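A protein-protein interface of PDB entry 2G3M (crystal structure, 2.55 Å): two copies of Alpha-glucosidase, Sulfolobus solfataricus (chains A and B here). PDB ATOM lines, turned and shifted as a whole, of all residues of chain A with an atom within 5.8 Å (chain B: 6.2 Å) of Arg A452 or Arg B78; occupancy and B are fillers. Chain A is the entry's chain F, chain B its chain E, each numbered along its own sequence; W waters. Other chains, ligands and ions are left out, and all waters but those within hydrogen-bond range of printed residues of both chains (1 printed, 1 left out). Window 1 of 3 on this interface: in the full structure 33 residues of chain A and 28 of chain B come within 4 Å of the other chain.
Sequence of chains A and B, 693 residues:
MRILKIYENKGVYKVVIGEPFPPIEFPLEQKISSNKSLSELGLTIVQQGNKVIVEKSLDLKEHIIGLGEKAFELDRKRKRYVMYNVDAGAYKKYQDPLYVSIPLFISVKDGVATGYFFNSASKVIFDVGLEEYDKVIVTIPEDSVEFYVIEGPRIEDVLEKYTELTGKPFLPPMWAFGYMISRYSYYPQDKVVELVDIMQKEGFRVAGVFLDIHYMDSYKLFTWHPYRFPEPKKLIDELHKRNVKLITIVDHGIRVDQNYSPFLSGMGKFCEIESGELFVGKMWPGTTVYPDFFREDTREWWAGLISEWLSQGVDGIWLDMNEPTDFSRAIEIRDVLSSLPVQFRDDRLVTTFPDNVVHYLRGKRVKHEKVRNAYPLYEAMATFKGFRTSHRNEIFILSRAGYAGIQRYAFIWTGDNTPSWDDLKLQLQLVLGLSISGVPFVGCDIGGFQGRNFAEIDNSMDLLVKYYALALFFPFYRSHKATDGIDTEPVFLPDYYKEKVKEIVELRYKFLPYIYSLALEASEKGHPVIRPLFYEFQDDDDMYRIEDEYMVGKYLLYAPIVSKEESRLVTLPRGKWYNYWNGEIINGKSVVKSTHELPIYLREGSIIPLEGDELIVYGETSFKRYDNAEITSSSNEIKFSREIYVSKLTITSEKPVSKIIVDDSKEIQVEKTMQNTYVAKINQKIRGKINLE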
ATOM      1  N   ARG A 183      20.604 -12.724  23.213  1.00  0.00           N
ATOM      2  CA  ARG A 183      20.619 -11.771  22.132  1.00  0.00           C
ATOM      3  C   ARG A 183      19.371 -11.991  21.315  1.00  0.00           C
ATOM      4  O   ARG A 183      18.693 -13.004  21.451  1.00  0.00           O
ATOM      5  CB  ARG A 183      21.855 -11.940  21.245  1.00  0.00           C
ATOM      6  CG  ARG A 183      22.013 -10.802  20.228  1.00  0.00           C
ATOM      7  CD  ARG A 183      23.217 -10.973  19.312  1.00  0.00           C
ATOM      8  NE  ARG A 183      23.247  -9.950  18.265  1.00  0.00           N
ATOM      9  CZ  ARG A 183      23.784  -8.740  18.396  1.00  0.00           C
ATOM     10  NH1 ARG A 183      24.360  -8.374  19.532  1.00  0.00           N
ATOM     11  NH2 ARG A 183      23.727  -7.880  17.391  1.00  0.00           N
ATOM     12  N   GLN A 450      18.400  -1.836  23.396  1.00  0.00           N
ATOM     13  CA  GLN A 450      18.477  -1.086  22.145  1.00  0.00           C
ATOM     14  C   GLN A 450      19.843  -1.208  21.462  1.00  0.00           C
ATOM     15  O   GLN A 450      20.896  -1.095  22.104  1.00  0.00           O
ATOM     16  CB  GLN A 450      18.144   0.391  22.379  1.00  0.00           C
ATOM     17  CG  GLN A 450      16.762   0.666  22.985  1.00  0.00           C
ATOM     18  CD  GLN A 450      15.615   0.062  22.185  1.00  0.00           C
ATOM     19  OE1 GLN A 450      15.671  -0.026  20.951  1.00  0.00           O
ATOM     20  NE2 GLN A 450      14.554  -0.341  22.885  1.00  0.00           N
ATOM     21  N   GLY A 451      19.811  -1.436  20.152  1.00  0.00           N
ATOM     22  CA  GLY A 451      21.037  -1.597  19.396  1.00  0.00           C
ATOM     23  C   GLY A 451      21.587  -0.315  18.820  1.00  0.00           C
ATOM     24  O   GLY A 451      22.367   0.376  19.468  1.00  0.00           O
ATOM     25  N   ARG A 452      21.193  -0.002  17.591  1.00  0.00           N
ATOM     26  CA  ARG A 452      21.661   1.215  16.938  1.00  0.00           C
ATOM     27  C   ARG A 452      20.618   1.767  15.981  1.00  0.00           C
ATOM     28  O   ARG A 452      20.961   2.221  14.898  1.00  0.00           O
ATOM     29  CB  ARG A 452      22.956   0.948  16.157  1.00  0.00           C
ATOM     30  CG  ARG A 452      24.160   0.600  17.011  1.00  0.00           C
ATOM     31  CD  ARG A 452      24.733  -0.717  16.551  1.00  0.00           C
ATOM     32  NE  ARG A 452      26.023  -0.567  15.895  1.00  0.00           N
ATOM     33  CZ  ARG A 452      26.538  -1.455  15.053  1.00  0.00           C
ATOM     34  NH1 ARG A 452      25.874  -2.560  14.748  1.00  0.00           N
ATOM     35  NH2 ARG A 452      27.733  -1.243  14.527  1.00  0.00           N
ATOM     36  N   ASN A 453      19.349   1.733  16.374  1.00  0.00           N
ATOM     37  CA  ASN A 453      18.298   2.235  15.498  1.00  0.00           C
ATOM     38  C   ASN A 453      17.965   3.714  15.699  1.00  0.00           C
ATOM     39  O   ASN A 453      17.100   4.255  15.014  1.00  0.00           O
ATOM     40  CB  ASN A 453      17.041   1.370  15.610  1.00  0.00           C
ATOM     41  CG  ASN A 453      16.578   1.201  17.037  1.00  0.00           C
ATOM     42  OD1 ASN A 453      17.372   0.884  17.933  1.00  0.00           O
ATOM     43  ND2 ASN A 453      15.285   1.398  17.260  1.00  0.00           N
ATOM     44  N   PHE A 454      18.640   4.358  16.650  1.00  0.00           N
ATOM     45  CA  PHE A 454      18.491   5.795  16.873  1.00  0.00           C
ATOM     46  C   PHE A 454      19.771   6.314  17.515  1.00  0.00           C
ATOM     47  O   PHE A 454      20.522   5.547  18.119  1.00  0.00           O
ATOM     48  CB  PHE A 454      17.238   6.169  17.695  1.00  0.00           C
ATOM     49  CG  PHE A 454      17.100   5.457  19.015  1.00  0.00           C
ATOM     50  CD1 PHE A 454      16.558   4.178  19.078  1.00  0.00           C
ATOM     51  CD2 PHE A 454      17.448   6.095  20.199  1.00  0.00           C
ATOM     52  CE1 PHE A 454      16.360   3.548  20.304  1.00  0.00           C
ATOM     53  CE2 PHE A 454      17.255   5.473  21.434  1.00  0.00           C
ATOM     54  CZ  PHE A 454      16.709   4.199  21.489  1.00  0.00           C
ATOM     55  N   ILE A 457      21.965   6.325  21.722  1.00  0.00           N
ATOM     56  CA  ILE A 457      22.326   5.033  22.291  1.00  0.00           C
ATOM     57  C   ILE A 457      23.829   5.042  22.540  1.00  0.00           C
ATOM     58  O   ILE A 457      24.618   5.269  21.616  1.00  0.00           O
ATOM     59  CB  ILE A 457      21.979   3.881  21.335  1.00  0.00           C
ATOM     60  CG1 ILE A 457      20.472   3.872  21.065  1.00  0.00           C
ATOM     61  CG2 ILE A 457      22.430   2.551  21.938  1.00  0.00           C
ATOM     62  CD1 ILE A 457      20.014   2.793  20.103  1.00  0.00           C
ATOM     63  N   ASN A 459      26.963   2.973  23.317  1.00  0.00           N
ATOM     64  CA  ASN A 459      27.541   1.630  23.313  1.00  0.00           C
ATOM     65  C   ASN A 459      29.002   1.594  23.770  1.00  0.00           C
ATOM     66  O   ASN A 459      29.731   0.655  23.454  1.00  0.00           O
ATOM     67  CB  ASN A 459      27.430   1.012  21.915  1.00  0.00           C
ATOM     68  CG  ASN A 459      26.000   0.659  21.545  1.00  0.00           C
ATOM     69  OD1 ASN A 459      25.341  -0.122  22.237  1.00  0.00           O
ATOM     70  ND2 ASN A 459      25.515   1.224  20.448  1.00  0.00           N
ATOM     71  N   THR A 483      18.948  -6.950  17.665  1.00  0.00           N
ATOM     72  CA  THR A 483      19.598  -7.469  16.469  1.00  0.00           C
ATOM     73  C   THR A 483      20.694  -6.602  15.851  1.00  0.00           C
ATOM     74  O   THR A 483      21.752  -7.117  15.475  1.00  0.00           O
ATOM     75  CB  THR A 483      18.567  -7.766  15.372  1.00  0.00           C
ATOM     76  OG1 THR A 483      17.356  -8.242  15.969  1.00  0.00           O
ATOM     77  CG2 THR A 483      19.090  -8.850  14.441  1.00  0.00           C
ATOM     78  N   ASP A 484      20.447  -5.299  15.746  1.00  0.00           N
ATOM     79  CA  ASP A 484      21.415  -4.395  15.135  1.00  0.00           C
ATOM     80  C   ASP A 484      22.403  -3.784  16.114  1.00  0.00           C
ATOM     81  O   ASP A 484      23.120  -2.848  15.772  1.00  0.00           O
ATOM     82  CB  ASP A 484      20.687  -3.282  14.370  1.00  0.00           C
ATOM     83  CG  ASP A 484      20.060  -2.236  15.288  1.00  0.00           C
ATOM     84  OD1 ASP A 484      19.592  -2.588  16.392  1.00  0.00           O
ATOM     85  OD2 ASP A 484      20.019  -1.049  14.890  1.00  0.00           O
ATOM     86  N   GLY A 485      22.444  -4.304  17.335  1.00  0.00           N
ATOM     87  CA  GLY A 485      23.384  -3.780  18.305  1.00  0.00           C
ATOM     88  C   GLY A 485      24.736  -4.436  18.111  1.00  0.00           C
ATOM     89  O   GLY A 485      24.832  -5.499  17.498  1.00  0.00           O
ATOM     90  N   ILE A 486      25.788  -3.803  18.611  1.00  0.00           N
ATOM     91  CA  ILE A 486      27.127  -4.370  18.497  1.00  0.00           C
ATOM     92  C   ILE A 486      27.148  -5.623  19.360  1.00  0.00           C
ATOM     93  O   ILE A 486      26.276  -5.799  20.213  1.00  0.00           O
ATOM     94  CB  ILE A 486      28.191  -3.399  19.040  1.00  0.00           C
ATOM     95  CG1 ILE A 486      27.883  -3.070  20.504  1.00  0.00           C
ATOM     96  CG2 ILE A 486      28.215  -2.122  18.211  1.00  0.00           C
ATOM     97  CD1 ILE A 486      28.954  -2.247  21.190  1.00  0.00           C
ATOM     98  N   ASP A 487      28.128  -6.494  19.138  1.00  0.00           N
ATOM     99  CA  ASP A 487      28.247  -7.715  19.939  1.00  0.00           C
ATOM    100  C   ASP A 487      28.708  -7.287  21.330  1.00  0.00           C
ATOM    101  O   ASP A 487      29.749  -6.651  21.465  1.00  0.00           O
ATOM    102  CB  ASP A 487      29.277  -8.665  19.321  1.00  0.00           C
ATOM    103  CG  ASP A 487      28.903  -9.097  17.913  1.00  0.00           C
ATOM    104  OD1 ASP A 487      27.812  -9.680  17.738  1.00  0.00           O
ATOM    105  OD2 ASP A 487      29.703  -8.857  16.977  1.00  0.00           O
ATOM    106  N   LEU B  58      30.101 -15.627   7.655  1.00  0.00           N
ATOM    107  CA  LEU B  58      30.655 -14.670   8.601  1.00  0.00           C
ATOM    108  C   LEU B  58      30.895 -15.395   9.925  1.00  0.00           C
ATOM    109  O   LEU B  58      29.949 -15.868  10.558  1.00  0.00           O
ATOM    110  CB  LEU B  58      29.672 -13.510   8.802  1.00  0.00           C
ATOM    111  CG  LEU B  58      30.045 -12.417   9.800  1.00  0.00           C
ATOM    112  CD1 LEU B  58      31.255 -11.650   9.294  1.00  0.00           C
ATOM    113  CD2 LEU B  58      28.855 -11.483   9.991  1.00  0.00           C
ATOM    114  N   ASP B  59      32.151 -15.499  10.339  1.00  0.00           N
ATOM    115  CA  ASP B  59      32.455 -16.176  11.593  1.00  0.00           C
ATOM    116  C   ASP B  59      32.355 -15.218  12.766  1.00  0.00           C
ATOM    117  O   ASP B  59      32.370 -14.001  12.579  1.00  0.00           O
ATOM    118  CB  ASP B  59      33.858 -16.785  11.556  1.00  0.00           C
ATOM    119  CG  ASP B  59      34.051 -17.739  10.392  1.00  0.00           C
ATOM    120  OD1 ASP B  59      33.076 -18.430  10.005  1.00  0.00           O
ATOM    121  OD2 ASP B  59      35.186 -17.805   9.871  1.00  0.00           O
ATOM    122  N   LEU B  60      32.255 -15.775  13.971  1.00  0.00           N
ATOM    123  CA  LEU B  60      32.142 -14.976  15.185  1.00  0.00           C
ATOM    124  C   LEU B  60      33.289 -14.002  15.395  1.00  0.00           C
ATOM    125  O   LEU B  60      33.075 -12.873  15.835  1.00  0.00           O
ATOM    126  CB  LEU B  60      32.042 -15.881  16.417  1.00  0.00           C
ATOM    127  CG  LEU B  60      30.722 -16.614  16.638  1.00  0.00           C
ATOM    128  CD1 LEU B  60      30.827 -17.423  17.922  1.00  0.00           C
ATOM    129  CD2 LEU B  60      29.567 -15.607  16.718  1.00  0.00           C
ATOM    130  N   PHE B  72      28.973   4.643  12.062  1.00  0.00           N
ATOM    131  CA  PHE B  72      28.951   3.457  12.905  1.00  0.00           C
ATOM    132  C   PHE B  72      30.348   3.027  13.320  1.00  0.00           C
ATOM    133  O   PHE B  72      31.354   3.556  12.835  1.00  0.00           O
ATOM    134  CB  PHE B  72      28.304   2.286  12.155  1.00  0.00           C
ATOM    135  CG  PHE B  72      26.837   2.448  11.914  1.00  0.00           C
ATOM    136  CD1 PHE B  72      26.372   3.299  10.917  1.00  0.00           C
ATOM    137  CD2 PHE B  72      25.913   1.765  12.705  1.00  0.00           C
ATOM    138  CE1 PHE B  72      25.000   3.475  10.708  1.00  0.00           C
ATOM    139  CE2 PHE B  72      24.540   1.933  12.507  1.00  0.00           C
ATOM    140  CZ  PHE B  72      24.083   2.791  11.505  1.00  0.00           C
ATOM    141  N   GLU B  73      30.400   2.052  14.218  1.00  0.00           N
ATOM    142  CA  GLU B  73      31.664   1.502  14.684  1.00  0.00           C
ATOM    143  C   GLU B  73      32.456   0.977  13.472  1.00  0.00           C
ATOM    144  O   GLU B  73      31.873   0.518  12.484  1.00  0.00           O
ATOM    145  CB  GLU B  73      31.405   0.354  15.665  1.00  0.00           C
ATOM    146  CG  GLU B  73      30.824   0.764  17.020  1.00  0.00           C
ATOM    147  CD  GLU B  73      29.381   1.265  16.951  1.00  0.00           C
ATOM    148  OE1 GLU B  73      28.688   1.011  15.939  1.00  0.00           O
ATOM    149  OE2 GLU B  73      28.934   1.902  17.928  1.00  0.00           O
ATOM    150  N   ASP B  75      34.151  -1.747  13.032  1.00  0.00           N
ATOM    151  CA  ASP B  75      33.871  -3.148  12.706  1.00  0.00           C
ATOM    152  C   ASP B  75      32.377  -3.075  12.392  1.00  0.00           C
ATOM    153  O   ASP B  75      31.568  -2.829  13.283  1.00  0.00           O
ATOM    154  CB  ASP B  75      34.117  -4.063  13.905  1.00  0.00           C
ATOM    155  CG  ASP B  75      34.302  -5.521  13.497  1.00  0.00           C
ATOM    156  OD1 ASP B  75      33.605  -5.980  12.558  1.00  0.00           O
ATOM    157  OD2 ASP B  75      35.138  -6.215  14.129  1.00  0.00           O
ATOM    158  N   ARG B  76      32.026  -3.296  11.128  1.00  0.00           N
ATOM    159  CA  ARG B  76      30.654  -3.158  10.637  1.00  0.00           C
ATOM    160  C   ARG B  76      29.577  -4.193  10.947  1.00  0.00           C
ATOM    161  O   ARG B  76      28.418  -3.989  10.588  1.00  0.00           O
ATOM    162  CB  ARG B  76      30.688  -2.956   9.118  1.00  0.00           C
ATOM    163  CG  ARG B  76      31.692  -1.919   8.633  1.00  0.00           C
ATOM    164  CD  ARG B  76      31.498  -0.552   9.286  1.00  0.00           C
ATOM    165  NE  ARG B  76      32.194   0.479   8.517  1.00  0.00           N
ATOM    166  CZ  ARG B  76      32.398   1.730   8.917  1.00  0.00           C
ATOM    167  NH1 ARG B  76      31.963   2.142  10.100  1.00  0.00           N
ATOM    168  NH2 ARG B  76      33.036   2.576   8.118  1.00  0.00           N
ATOM    169  N   LYS B  77      29.930  -5.282  11.608  1.00  0.00           N
ATOM    170  CA  LYS B  77      28.962  -6.326  11.909  1.00  0.00           C
ATOM    171  C   LYS B  77      27.657  -5.905  12.590  1.00  0.00           C
ATOM    172  O   LYS B  77      27.606  -4.930  13.335  1.00  0.00           O
ATOM    173  CB  LYS B  77      29.646  -7.426  12.726  1.00  0.00           C
ATOM    174  CG  LYS B  77      30.624  -8.248  11.896  1.00  0.00           C
ATOM    175  CD  LYS B  77      31.731  -8.853  12.739  1.00  0.00           C
ATOM    176  CE  LYS B  77      31.199  -9.878  13.718  1.00  0.00           C
ATOM    177  NZ  LYS B  77      32.285 -10.332  14.632  1.00  0.00           N
ATOM    178  N   ARG B  78      26.605  -6.668  12.303  1.00  0.00           N
ATOM    179  CA  ARG B  78      25.269  -6.476  12.859  1.00  0.00           C
ATOM    180  C   ARG B  78      24.531  -5.236  12.367  1.00  0.00           C
ATOM    181  O   ARG B  78      23.897  -4.534  13.153  1.00  0.00           O
ATOM    182  CB  ARG B  78      25.333  -6.457  14.391  1.00  0.00           C
ATOM    183  CG  ARG B  78      26.185  -7.568  15.003  1.00  0.00           C
ATOM    184  CD  ARG B  78      25.846  -8.937  14.435  1.00  0.00           C
ATOM    185  NE  ARG B  78      26.851  -9.920  14.827  1.00  0.00           N
ATOM    186  CZ  ARG B  78      27.084 -11.061  14.183  1.00  0.00           C
ATOM    187  NH1 ARG B  78      26.382 -11.372  13.101  1.00  0.00           N
ATOM    188  NH2 ARG B  78      28.019 -11.893  14.625  1.00  0.00           N
ATOM    189  N   LYS B  79      24.602  -4.976  11.065  1.00  0.00           N
ATOM    190  CA  LYS B  79      23.923  -3.824  10.497  1.00  0.00           C
ATOM    191  C   LYS B  79      23.693  -4.013   9.004  1.00  0.00           C
ATOM    192  O   LYS B  79      24.479  -4.671   8.330  1.00  0.00           O
ATOM    193  CB  LYS B  79      24.752  -2.562  10.728  1.00  0.00           C
ATOM    194  CG  LYS B  79      24.023  -1.282  10.379  1.00  0.00           C
ATOM    195  CD  LYS B  79      22.825  -1.098  11.299  1.00  0.00           C
ATOM    196  CE  LYS B  79      22.007   0.147  10.959  1.00  0.00           C
ATOM    197  NZ  LYS B  79      20.948   0.375  12.006  1.00  0.00           N
ATOM    198  N   ARG B  80      22.603  -3.449   8.497  1.00  0.00           N
ATOM    199  CA  ARG B  80      22.277  -3.526   7.079  1.00  0.00           C
ATOM    200  C   ARG B  80      22.540  -2.122   6.532  1.00  0.00           C
ATOM    201  O   ARG B  80      21.778  -1.196   6.789  1.00  0.00           O
ATOM    202  CB  ARG B  80      20.804  -3.915   6.904  1.00  0.00           C
ATOM    203  CG  ARG B  80      20.357  -4.246   5.473  1.00  0.00           C
ATOM    204  CD  ARG B  80      18.865  -4.585   5.457  1.00  0.00           C
ATOM    205  NE  ARG B  80      18.324  -4.832   4.121  1.00  0.00           N
ATOM    206  CZ  ARG B  80      18.440  -5.976   3.452  1.00  0.00           C
ATOM    207  NH1 ARG B  80      19.085  -7.003   3.984  1.00  0.00           N
ATOM    208  NH2 ARG B  80      17.896  -6.096   2.249  1.00  0.00           N
ATOM    209  N   TYR B  81      23.633  -1.966   5.792  1.00  0.00           N
ATOM    210  CA  TYR B  81      24.000  -0.665   5.244  1.00  0.00           C
ATOM    211  C   TYR B  81      23.456  -0.395   3.842  1.00  0.00           C
ATOM    212  O   TYR B  81      23.390  -1.284   2.994  1.00  0.00           O
ATOM    213  CB  TYR B  81      25.527  -0.505   5.219  1.00  0.00           C
ATOM    214  CG  TYR B  81      26.203  -0.732   6.553  1.00  0.00           C
ATOM    215  CD1 TYR B  81      26.560  -2.018   6.969  1.00  0.00           C
ATOM    216  CD2 TYR B  81      26.469   0.335   7.412  1.00  0.00           C
ATOM    217  CE1 TYR B  81      27.163  -2.231   8.204  1.00  0.00           C
ATOM    218  CE2 TYR B  81      27.069   0.130   8.649  1.00  0.00           C
ATOM    219  CZ  TYR B  81      27.414  -1.154   9.039  1.00  0.00           C
ATOM    220  OH  TYR B  81      28.001  -1.365  10.266  1.00  0.00           O
ATOM    221  N   LYS B  93      24.696  10.193  14.972  1.00  0.00           N
ATOM    222  CA  LYS B  93      25.315   8.892  14.825  1.00  0.00           C
ATOM    223  C   LYS B  93      24.274   7.818  14.546  1.00  0.00           C
ATOM    224  O   LYS B  93      23.104   7.945  14.928  1.00  0.00           O
ATOM    225  CB  LYS B  93      26.168   8.533  16.044  1.00  0.00           C
ATOM    226  CG  LYS B  93      25.443   8.236  17.325  1.00  0.00           C
ATOM    227  CD  LYS B  93      26.447   7.612  18.291  1.00  0.00           C
ATOM    228  CE  LYS B  93      25.886   7.437  19.684  1.00  0.00           C
ATOM    229  NZ  LYS B  93      26.854   6.687  20.535  1.00  0.00           N
ATOM    230  N   TYR B  94      24.714   6.778  13.849  1.00  0.00           N
ATOM    231  CA  TYR B  94      23.869   5.660  13.462  1.00  0.00           C
ATOM    232  C   TYR B  94      22.892   6.010  12.345  1.00  0.00           C
ATOM    233  O   TYR B  94      21.988   5.244  12.036  1.00  0.00           O
ATOM    234  CB  TYR B  94      23.122   5.096  14.674  1.00  0.00           C
ATOM    235  CG  TYR B  94      24.050   4.576  15.749  1.00  0.00           C
ATOM    236  CD1 TYR B  94      25.283   3.996  15.418  1.00  0.00           C
ATOM    237  CD2 TYR B  94      23.702   4.657  17.095  1.00  0.00           C
ATOM    238  CE1 TYR B  94      26.139   3.516  16.398  1.00  0.00           C
ATOM    239  CE2 TYR B  94      24.550   4.171  18.082  1.00  0.00           C
ATOM    240  CZ  TYR B  94      25.764   3.606  17.731  1.00  0.00           C
ATOM    241  OH  TYR B  94      26.589   3.135  18.729  1.00  0.00           O
ATOM    242  N   VAL B 128      25.473  -6.997   6.806  1.00  0.00           N
ATOM    243  CA  VAL B 128      26.557  -7.636   7.542  1.00  0.00           C
ATOM    244  C   VAL B 128      26.117  -8.348   8.821  1.00  0.00           C
ATOM    245  O   VAL B 128      26.089  -7.760   9.896  1.00  0.00           O
ATOM    246  CB  VAL B 128      27.635  -6.590   7.883  1.00  0.00           C
ATOM    247  CG1 VAL B 128      28.892  -7.273   8.391  1.00  0.00           C
ATOM    248  CG2 VAL B 128      27.933  -5.746   6.646  1.00  0.00           C
ATOM    249  N   GLY B 129      25.773  -9.623   8.692  1.00  0.00           N
ATOM    250  CA  GLY B 129      25.350 -10.403   9.841  1.00  0.00           C
ATOM    251  C   GLY B 129      24.103  -9.905  10.542  1.00  0.00           C
ATOM    252  O   GLY B 129      23.960 -10.086  11.745  1.00  0.00           O
ATOM    253  N   LEU B 130      23.196  -9.278   9.801  1.00  0.00           N
ATOM    254  CA  LEU B 130      21.962  -8.767  10.389  1.00  0.00           C
ATOM    255  C   LEU B 130      20.810  -9.696  10.010  1.00  0.00           C
ATOM    256  O   LEU B 130      20.148 -10.262  10.879  1.00  0.00           O
ATOM    257  CB  LEU B 130      21.698  -7.343   9.886  1.00  0.00           C
ATOM    258  CG  LEU B 130      20.830  -6.377  10.705  1.00  0.00           C
ATOM    259  CD1 LEU B 130      19.504  -6.177  10.020  1.00  0.00           C
ATOM    260  CD2 LEU B 130      20.651  -6.884  12.126  1.00  0.00           C
ATOM    261  N   GLU B 132      21.075 -12.550   8.467  1.00  0.00           N
ATOM    262  CA  GLU B 132      21.537 -13.873   8.837  1.00  0.00           C
ATOM    263  C   GLU B 132      22.812 -13.655   9.657  1.00  0.00           C
ATOM    264  O   GLU B 132      23.823 -13.178   9.152  1.00  0.00           O
ATOM    265  CB  GLU B 132      21.791 -14.687   7.566  1.00  0.00           C
ATOM    266  CG  GLU B 132      21.212 -16.100   7.592  1.00  0.00           C
ATOM    267  CD  GLU B 132      19.714 -16.156   7.916  1.00  0.00           C
ATOM    268  OE1 GLU B 132      18.904 -15.570   7.163  1.00  0.00           O
ATOM    269  OE2 GLU B 132      19.346 -16.799   8.925  1.00  0.00           O
ATOM    270  N   TYR B 133      22.730 -13.976  10.941  1.00  0.00           N
ATOM    271  CA  TYR B 133      23.829 -13.797  11.885  1.00  0.00           C
ATOM    272  C   TYR B 133      25.185 -14.309  11.415  1.00  0.00           C
ATOM    273  O   TYR B 133      26.212 -13.734  11.751  1.00  0.00           O
ATOM    274  CB  TYR B 133      23.475 -14.480  13.204  1.00  0.00           C
ATOM    275  CG  TYR B 133      24.372 -14.129  14.369  1.00  0.00           C
ATOM    276  CD1 TYR B 133      24.189 -12.943  15.082  1.00  0.00           C
ATOM    277  CD2 TYR B 133      25.375 -15.001  14.789  1.00  0.00           C
ATOM    278  CE1 TYR B 133      24.978 -12.637  16.195  1.00  0.00           C
ATOM    279  CE2 TYR B 133      26.171 -14.705  15.894  1.00  0.00           C
ATOM    280  CZ  TYR B 133      25.965 -13.524  16.595  1.00  0.00           C
ATOM    281  OH  TYR B 133      26.736 -13.251  17.709  1.00  0.00           O
ATOM    282  N   ASP B 134      25.182 -15.388  10.640  1.00  0.00           N
ATOM    283  CA  ASP B 134      26.421 -15.990  10.159  1.00  0.00           C
ATOM    284  C   ASP B 134      26.697 -15.705   8.692  1.00  0.00           C
ATOM    285  O   ASP B 134      27.405 -16.467   8.032  1.00  0.00           O
ATOM    286  CB  ASP B 134      26.378 -17.506  10.387  1.00  0.00           C
ATOM    287  CG  ASP B 134      25.293 -18.194   9.567  1.00  0.00           C
ATOM    288  OD1 ASP B 134      24.255 -17.556   9.275  1.00  0.00           O
ATOM    289  OD2 ASP B 134      25.467 -19.384   9.229  1.00  0.00           O
ATOM    290  N   LYS B 135      26.161 -14.603   8.179  1.00  0.00           N
ATOM    291  CA  LYS B 135      26.371 -14.270   6.779  1.00  0.00           C
ATOM    292  C   LYS B 135      26.462 -12.797   6.428  1.00  0.00           C
ATOM    293  O   LYS B 135      25.916 -11.938   7.115  1.00  0.00           O
ATOM    294  CB  LYS B 135      25.261 -14.900   5.939  1.00  0.00           C
ATOM    295  CG  LYS B 135      25.491 -16.352   5.625  1.00  0.00           C
ATOM    296  CD  LYS B 135      24.232 -17.020   5.111  1.00  0.00           C
ATOM    297  CE  LYS B 135      24.545 -18.427   4.603  1.00  0.00           C
ATOM    298  NZ  LYS B 135      25.495 -19.139   5.514  1.00  0.00           N
HETATM  299  O   HOH W   1      28.024   4.376  21.266  1.00  0.00           O
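The side-chain carboxylate of Glu B73 is in salt-bridge range of the guanidinium group of Arg A452 (2.8 Å).
The guanidinium group (NH1) of Arg A452 lies within hydrogen-bond range of the backbone carbonyl oxygen (O) of Lys B77 (3.3 Å).
The guanidinium group (NE) of Arg B78 lies within salt-bridge range of the side-chain carboxylate (OD1) of Asp A487 (3.1 Å).
The side-chain amino group (NZ) of Lys B79 sits at hydrogen-bond distance from the backbone carbonyl oxygen (O) of Arg A452.
The side-chain carboxylate of Asp A484 is in salt-bridge range of the side-chain amino group of Lys B79, 3.3 Å away.
The side-chain amino group (NZ) of Lys B93 lies within hydrogen-bond range of the backbone carbonyl oxygen (O) of Ile A457, at 2.9 Å.
O of Asp A484 lies close to O of Arg B78, at 3.2 Å.
The guanidinium group of Arg B78 is in hydrogen-bond range of the backbone carbonyl oxygen of Tyr B133 (2.7 Å).
The backbone NH of Val B128 sits at hydrogen-bond distance from the backbone carbonyl oxygen of Lys B79 (3.0 Å).
NH2 of Arg A183 touches CG of Arg B78, at 3.4 Å.
Phe B72 touches Arg A452.
CB of Arg B78 touches O of Thr A483, 3.8 Å away.
Arg B78 touches Gly A485 (CB to O, 3.3 Å).
Ile A486 touches Glu B73.
Tyr B133 touches Asp A487.
Of the printed residues of chain B, Asp A484 touches Arg B78 (3.2 Å), Lys B79 (3.3 Å) and Leu B130 (3.96 Å).
Of chain A, only Arg A183, Arg A452, Thr A483, Asp A484, Gly A485 and Asp A487 come within 4 Å of Arg B78.
Printed residues of chain A within 4 Å of Lys B93: Ile A457 (2.9 Å).
The nearest residue of chain A that does not touch Arg B78 is Ile A486 (4.8 Å).
The nearest printed residue of chain B that does not touch Ile A486 is Arg B78 (4.8 Å).
Of the 13 printed residues of chain A, 10 touch a printed residue of chain B.
Printed residues of chain A that touch a printed residue of chain B: Arg A183, Arg A452, Phe A454, Ile A457, Asn A459, Thr A483, Asp A484, Gly A485, Ile A486 and Asp A487.
Hydrophobic or aromatic side chains of chain B within 4 Å of the printed part of chain A: Phe B72, Tyr B94, Leu B130 and Tyr B133.
Among the printed residues, Asp or Glu carboxylates within 4 Å of a Lys or Arg side-chain nitrogen of the other chain: Arg A452 with Glu B73 (2.8 Å), Asp A484 with Lys B79 (3.3 Å), Asp A487 with Lys B77 (3.8 Å) and Asp A487 with Arg B78 (3.1 Å).
No position is printed for both chains.
Water W1 lies within hydrogen-bond range of NZ of Lys B93, N of Asn A459 and OH of Tyr B94.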
